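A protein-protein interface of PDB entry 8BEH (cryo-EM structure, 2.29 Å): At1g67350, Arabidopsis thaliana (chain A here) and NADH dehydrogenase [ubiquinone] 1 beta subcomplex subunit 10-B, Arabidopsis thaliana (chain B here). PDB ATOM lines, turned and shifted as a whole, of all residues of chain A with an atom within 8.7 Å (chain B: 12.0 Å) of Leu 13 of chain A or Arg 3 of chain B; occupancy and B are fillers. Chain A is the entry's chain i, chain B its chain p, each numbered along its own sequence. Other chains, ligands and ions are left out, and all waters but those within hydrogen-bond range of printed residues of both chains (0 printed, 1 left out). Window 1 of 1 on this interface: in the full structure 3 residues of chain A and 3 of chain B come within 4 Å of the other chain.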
ATOM      1  N   GLU A   6       9.758  30.335  14.096  1.00  0.00           N
ATOM      2  CA  GLU A   6      10.691  29.373  14.716  1.00  0.00           C
ATOM      3  C   GLU A   6      10.722  29.665  16.224  1.00  0.00           C
ATOM      4  O   GLU A   6      10.576  28.717  16.988  1.00  0.00           O
ATOM      5  CB  GLU A   6      12.045  29.334  14.006  1.00  0.00           C
ATOM      6  CG  GLU A   6      13.033  28.399  14.673  1.00  0.00           C
ATOM      7  CD  GLU A   6      14.494  28.734  14.437  1.00  0.00           C
ATOM      8  OE1 GLU A   6      14.776  29.869  13.999  1.00  0.00           O
ATOM      9  OE2 GLU A   6      15.348  27.864  14.698  1.00  0.00           O
ATOM     10  N   PHE A   7      10.775  30.928  16.597  1.00  0.00           N
ATOM     11  CA  PHE A   7      10.722  31.301  18.028  1.00  0.00           C
ATOM     12  C   PHE A   7       9.410  30.752  18.604  1.00  0.00           C
ATOM     13  O   PHE A   7       9.452  30.228  19.674  1.00  0.00           O
ATOM     14  CB  PHE A   7      10.935  32.814  18.197  1.00  0.00           C
ATOM     15  CG  PHE A   7      10.534  33.341  19.543  1.00  0.00           C
ATOM     16  CD1 PHE A   7       9.212  33.645  19.818  1.00  0.00           C
ATOM     17  CD2 PHE A   7      11.472  33.485  20.544  1.00  0.00           C
ATOM     18  CE1 PHE A   7       8.843  34.097  21.069  1.00  0.00           C
ATOM     19  CE2 PHE A   7      11.101  33.942  21.791  1.00  0.00           C
ATOM     20  CZ  PHE A   7       9.790  34.251  22.052  1.00  0.00           C
ATOM     21  N   ALA A   8       8.298  30.948  17.890  1.00  0.00           N
ATOM     22  CA  ALA A   8       7.018  30.480  18.410  1.00  0.00           C
ATOM     23  C   ALA A   8       7.004  28.962  18.585  1.00  0.00           C
ATOM     24  O   ALA A   8       6.468  28.454  19.576  1.00  0.00           O
ATOM     25  CB  ALA A   8       5.884  30.937  17.496  1.00  0.00           C
ATOM     26  N   GLU A   9       7.584  28.226  17.630  1.00  0.00           N
ATOM     27  CA  GLU A   9       7.743  26.780  17.784  1.00  0.00           C
ATOM     28  C   GLU A   9       8.444  26.452  19.089  1.00  0.00           C
ATOM     29  O   GLU A   9       7.965  25.636  19.888  1.00  0.00           O
ATOM     30  CB  GLU A   9       8.562  26.172  16.640  1.00  0.00           C
ATOM     31  CG  GLU A   9       7.877  25.620  15.398  1.00  0.00           C
ATOM     32  CD  GLU A   9       7.037  26.593  14.617  1.00  0.00           C
ATOM     33  OE1 GLU A   9       7.613  27.422  13.889  1.00  0.00           O
ATOM     34  OE2 GLU A   9       5.809  26.470  14.649  1.00  0.00           O
ATOM     35  N   ASN A  10       9.595  27.083  19.310  1.00  0.00           N
ATOM     36  CA  ASN A  10      10.384  26.778  20.496  1.00  0.00           C
ATOM     37  C   ASN A  10       9.638  27.148  21.771  1.00  0.00           C
ATOM     38  O   ASN A  10       9.664  26.397  22.750  1.00  0.00           O
ATOM     39  CB  ASN A  10      11.733  27.486  20.418  1.00  0.00           C
ATOM     40  CG  ASN A  10      12.648  26.860  19.398  1.00  0.00           C
ATOM     41  OD1 ASN A  10      12.325  25.827  18.815  1.00  0.00           O
ATOM     42  ND2 ASN A  10      13.801  27.480  19.171  1.00  0.00           N
ATOM     43  N   LEU A  11       8.963  28.295  21.773  1.00  0.00           N
ATOM     44  CA  LEU A  11       8.225  28.722  22.958  1.00  0.00           C
ATOM     45  C   LEU A  11       7.096  27.750  23.286  1.00  0.00           C
ATOM     46  O   LEU A  11       6.909  27.363  24.448  1.00  0.00           O
ATOM     47  CB  LEU A  11       7.690  30.136  22.742  1.00  0.00           C
ATOM     48  CG  LEU A  11       6.859  30.771  23.852  1.00  0.00           C
ATOM     49  CD1 LEU A  11       7.525  30.584  25.207  1.00  0.00           C
ATOM     50  CD2 LEU A  11       6.632  32.231  23.549  1.00  0.00           C
ATOM     51  N   VAL A  12       6.338  27.330  22.269  1.00  0.00           N
ATOM     52  CA  VAL A  12       5.263  26.368  22.496  1.00  0.00           C
ATOM     53  C   VAL A  12       5.829  25.061  23.035  1.00  0.00           C
ATOM     54  O   VAL A  12       5.276  24.468  23.970  1.00  0.00           O
ATOM     55  CB  VAL A  12       4.452  26.143  21.206  1.00  0.00           C
ATOM     56  CG1 VAL A  12       3.543  24.935  21.363  1.00  0.00           C
ATOM     57  CG2 VAL A  12       3.634  27.373  20.864  1.00  0.00           C
ATOM     58  N   LEU A  13       6.943  24.596  22.461  1.00  0.00           N
ATOM     59  CA  LEU A  13       7.572  23.379  22.963  1.00  0.00           C
ATOM     60  C   LEU A  13       7.980  23.538  24.423  1.00  0.00           C
ATOM     61  O   LEU A  13       7.834  22.607  25.224  1.00  0.00           O
ATOM     62  CB  LEU A  13       8.783  23.026  22.103  1.00  0.00           C
ATOM     63  CG  LEU A  13       8.547  22.436  20.712  1.00  0.00           C
ATOM     64  CD1 LEU A  13       9.811  21.771  20.217  1.00  0.00           C
ATOM     65  CD2 LEU A  13       7.381  21.462  20.700  1.00  0.00           C
ATOM     66  N   ARG A  14       8.486  24.717  24.786  1.00  0.00           N
ATOM     67  CA  ARG A  14       8.834  24.991  26.176  1.00  0.00           C
ATOM     68  C   ARG A  14       7.615  24.881  27.082  1.00  0.00           C
ATOM     69  O   ARG A  14       7.704  24.350  28.192  1.00  0.00           O
ATOM     70  CB  ARG A  14       9.440  26.387  26.303  1.00  0.00           C
ATOM     71  CG  ARG A  14      10.941  26.444  26.375  1.00  0.00           C
ATOM     72  CD  ARG A  14      11.480  27.207  25.183  1.00  0.00           C
ATOM     73  NE  ARG A  14      11.081  28.608  25.241  1.00  0.00           N
ATOM     74  CZ  ARG A  14      11.281  29.490  24.272  1.00  0.00           C
ATOM     75  NH1 ARG A  14      11.878  29.151  23.142  1.00  0.00           N
ATOM     76  NH2 ARG A  14      10.862  30.742  24.437  1.00  0.00           N
ATOM     77  N   LEU A  15       6.467  25.392  26.627  1.00  0.00           N
ATOM     78  CA  LEU A  15       5.287  25.413  27.486  1.00  0.00           C
ATOM     79  C   LEU A  15       4.688  24.026  27.686  1.00  0.00           C
ATOM     80  O   LEU A  15       4.009  23.790  28.690  1.00  0.00           O
ATOM     81  CB  LEU A  15       4.234  26.357  26.910  1.00  0.00           C
ATOM     82  CG  LEU A  15       4.642  27.824  26.782  1.00  0.00           C
ATOM     83  CD1 LEU A  15       3.678  28.573  25.880  1.00  0.00           C
ATOM     84  CD2 LEU A  15       4.729  28.473  28.147  1.00  0.00           C
ATOM     85  N   MET A  16       4.920  23.105  26.760  1.00  0.00           N
ATOM     86  CA  MET A  16       4.265  21.802  26.805  1.00  0.00           C
ATOM     87  C   MET A  16       4.866  20.909  27.884  1.00  0.00           C
ATOM     88  O   MET A  16       4.180  20.065  28.455  1.00  0.00           O
ATOM     89  CB  MET A  16       4.355  21.118  25.443  1.00  0.00           C
ATOM     90  CG  MET A  16       3.462  21.734  24.385  1.00  0.00           C
ATOM     91  SD  MET A  16       3.325  20.729  22.899  1.00  0.00           S
ATOM     92  CE  MET A  16       1.816  21.364  22.185  1.00  0.00           C
ATOM     93  N   GLY B   2       8.525  20.565  29.419  1.00  0.00           N
ATOM     94  CA  GLY B   2       8.992  20.795  28.067  1.00  0.00           C
ATOM     95  C   GLY B   2       8.933  19.543  27.224  1.00  0.00           C
ATOM     96  O   GLY B   2       9.101  18.439  27.732  1.00  0.00           O
ATOM     97  N   ARG B   3       8.688  19.711  25.929  1.00  0.00           N
ATOM     98  CA  ARG B   3       8.568  18.596  25.007  1.00  0.00           C
ATOM     99  C   ARG B   3       9.579  18.757  23.879  1.00  0.00           C
ATOM    100  O   ARG B   3       9.761  19.854  23.344  1.00  0.00           O
ATOM    101  CB  ARG B   3       7.140  18.491  24.443  1.00  0.00           C
ATOM    102  CG  ARG B   3       7.066  18.059  22.993  1.00  0.00           C
ATOM    103  CD  ARG B   3       5.642  18.002  22.467  1.00  0.00           C
ATOM    104  NE  ARG B   3       4.839  16.993  23.145  1.00  0.00           N
ATOM    105  CZ  ARG B   3       4.798  15.715  22.800  1.00  0.00           C
ATOM    106  NH1 ARG B   3       5.522  15.247  21.797  1.00  0.00           N
ATOM    107  NH2 ARG B   3       4.014  14.886  23.478  1.00  0.00           N
ATOM    108  N   LYS B   4      10.237  17.658  23.533  1.00  0.00           N
ATOM    109  CA  LYS B   4      11.173  17.660  22.423  1.00  0.00           C
ATOM    110  C   LYS B   4      10.439  17.783  21.093  1.00  0.00           C
ATOM    111  O   LYS B   4       9.297  17.345  20.939  1.00  0.00           O
ATOM    112  CB  LYS B   4      12.012  16.386  22.440  1.00  0.00           C
ATOM    113  CG  LYS B   4      12.956  16.290  23.624  1.00  0.00           C
ATOM    114  CD  LYS B   4      13.745  14.993  23.602  1.00  0.00           C
ATOM    115  CE  LYS B   4      14.708  14.908  24.776  1.00  0.00           C
ATOM    116  NZ  LYS B   4      15.469  13.626  24.772  1.00  0.00           N
ATOM    117  N   LYS B   5      11.111  18.397  20.126  1.00  0.00           N
ATOM    118  CA  LYS B   5      10.557  18.500  18.788  1.00  0.00           C
ATOM    119  C   LYS B   5      10.440  17.116  18.165  1.00  0.00           C
ATOM    120  O   LYS B   5      11.299  16.255  18.364  1.00  0.00           O
ATOM    121  CB  LYS B   5      11.439  19.402  17.925  1.00  0.00           C
ATOM    122  CG  LYS B   5      10.984  19.540  16.486  1.00  0.00           C
ATOM    123  CD  LYS B   5      11.995  20.317  15.660  1.00  0.00           C
ATOM    124  CE  LYS B   5      11.306  21.233  14.668  1.00  0.00           C
ATOM    125  NZ  LYS B   5      10.299  22.109  15.331  1.00  0.00           N
ATOM    126  N   GLY B   6       9.359  16.894  17.428  1.00  0.00           N
ATOM    127  CA  GLY B   6       9.179  15.667  16.679  1.00  0.00           C
ATOM    128  C   GLY B   6       7.802  15.069  16.881  1.00  0.00           C
ATOM    129  O   GLY B   6       7.027  15.477  17.744  1.00  0.00           O
ATOM    130  N   LEU B   7       7.516  14.071  16.050  1.00  0.00           N
ATOM    131  CA  LEU B   7       6.257  13.353  16.148  1.00  0.00           C
ATOM    132  C   LEU B   7       6.191  12.556  17.450  1.00  0.00           C
ATOM    133  O   LEU B   7       7.220  12.162  17.999  1.00  0.00           O
ATOM    134  CB  LEU B   7       6.076  12.407  14.964  1.00  0.00           C
ATOM    135  CG  LEU B   7       5.572  12.997  13.650  1.00  0.00           C
ATOM    136  CD1 LEU B   7       6.681  13.708  12.876  1.00  0.00           C
ATOM    137  CD2 LEU B   7       4.909  11.916  12.812  1.00  0.00           C
ATOM    138  N   PRO B   8       4.987  12.307  17.964  1.00  0.00           N
ATOM    139  CA  PRO B   8       4.865  11.512  19.193  1.00  0.00           C
ATOM    140  C   PRO B   8       5.416  10.109  19.003  1.00  0.00           C
ATOM    141  O   PRO B   8       5.312   9.516  17.929  1.00  0.00           O
ATOM    142  CB  PRO B   8       3.355  11.482  19.466  1.00  0.00           C
ATOM    143  CG  PRO B   8       2.698  12.142  18.342  1.00  0.00           C
ATOM    144  CD  PRO B   8       3.693  12.764  17.436  1.00  0.00           C
ATOM    145  N   GLU B   9       6.004   9.575  20.066  1.00  0.00           N
ATOM    146  CA  GLU B   9       6.597   8.246  20.049  1.00  0.00           C
ATOM    147  C   GLU B   9       5.823   7.332  20.989  1.00  0.00           C
ATOM    148  O   GLU B   9       5.534   7.705  22.129  1.00  0.00           O
ATOM    149  CB  GLU B   9       8.069   8.288  20.456  1.00  0.00           C
ATOM    150  CG  GLU B   9       8.831   9.497  19.952  1.00  0.00           C
ATOM    151  CD  GLU B   9       8.692  10.690  20.880  1.00  0.00           C
ATOM    152  OE1 GLU B   9       8.847  10.505  22.105  1.00  0.00           O
ATOM    153  OE2 GLU B   9       8.427  11.805  20.391  1.00  0.00           O
ATOM    154  N   PHE B  10       5.526   6.155  20.509  1.00  0.00           N
ATOM    155  CA  PHE B  10       4.876   5.164  21.361  1.00  0.00           C
ATOM    156  C   PHE B  10       5.541   3.796  21.207  1.00  0.00           C
ATOM    157  O   PHE B  10       6.210   3.576  20.237  1.00  0.00           O
ATOM    158  CB  PHE B  10       3.385   5.099  21.054  1.00  0.00           C
ATOM    159  CG  PHE B  10       2.577   6.365  21.136  1.00  0.00           C
ATOM    160  CD1 PHE B  10       2.087   6.817  22.348  1.00  0.00           C
ATOM    161  CD2 PHE B  10       2.251   7.067  19.984  1.00  0.00           C
ATOM    162  CE1 PHE B  10       1.318   7.966  22.413  1.00  0.00           C
ATOM    163  CE2 PHE B  10       1.492   8.219  20.052  1.00  0.00           C
ATOM    164  CZ  PHE B  10       1.026   8.670  21.267  1.00  0.00           C
ATOM    165  N   ARG B  39      -4.625   3.097  19.150  1.00  0.00           N
ATOM    166  CA  ARG B  39      -3.605   3.464  18.172  1.00  0.00           C
ATOM    167  C   ARG B  39      -3.619   2.521  16.970  1.00  0.00           C
ATOM    168  O   ARG B  39      -3.498   2.964  15.819  1.00  0.00           O
ATOM    169  CB  ARG B  39      -2.235   3.488  18.846  1.00  0.00           C
ATOM    170  CG  ARG B  39      -1.661   4.885  19.004  1.00  0.00           C
ATOM    171  CD  ARG B  39      -1.222   5.212  20.412  1.00  0.00           C
ATOM    172  NE  ARG B  39      -0.437   4.159  21.041  1.00  0.00           N
ATOM    173  CZ  ARG B  39      -0.216   4.081  22.347  1.00  0.00           C
ATOM    174  NH1 ARG B  39      -0.704   4.980  23.183  1.00  0.00           N
ATOM    175  NH2 ARG B  39       0.510   3.077  22.825  1.00  0.00           N
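The backbone NH of Arg 3 of chain B sits at hydrogen-bond distance from the backbone carbonyl oxygen of Leu 13 of chain A (3.1 Å).
Among the printed residues, pairs that only touch across the chains: Leu 13 of chain A with Gly 2 of chain B (3.6 Å), Leu 13 of chain A with Lys 5 of chain B (3.6 Å), Arg 14 of chain A with Gly 2 of chain B (3.8 Å), Met 16 of chain A with Gly 2 of chain B (3.98 Å) and Met 16 of chain A with Arg 3 of chain B (3.6 Å).
Of the printed residues of chain B, Leu 13 of chain A touches Gly 2, Arg 3 and Lys 5.
Arg 3 of chain B touches two residues of chain A.
No residue of chain B comes within 4 Å of Asn 10 of chain A.
No residue of chain B comes within 4 Å of Leu 11 of chain A.
Arg 14 of chain A touches just one residue of chain B: Gly 2.
No residue of chain B comes within 4 Å of Leu 15 of chain A.
Of the printed residues of chain A, Lys 5 of chain B touches Leu 13.
Of the printed residues of chain A, Gly 2 of chain B touches Leu 13 (3.6 Å), Arg 14 (3.8 Å) and Met 16 (3.98 Å).
Of the printed residues of chain B, Met 16 of chain A touches Gly 2 and Arg 3.
Glu 9 of chain B touches none of the printed residues of chain A.
The nearest printed residue of chain A that does not touch Gly 2 of chain B is Leu 15 of chain A (5.4 Å).
Of the 10 printed residues of chain B, 3 touch a printed residue of chain A.
Printed residues of chain B that touch a printed residue of chain A: Gly 2, Arg 3 and Lys 5.
Of the 11 printed residues of chain A, 3 touch a printed residue of chain B.
Among the printed residues, 6 pairs touch across the chains.
Among the printed residues, no Asp or Glu carboxylate lies within 4 Å of a Lys or Arg side-chain nitrogen of the other chain.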
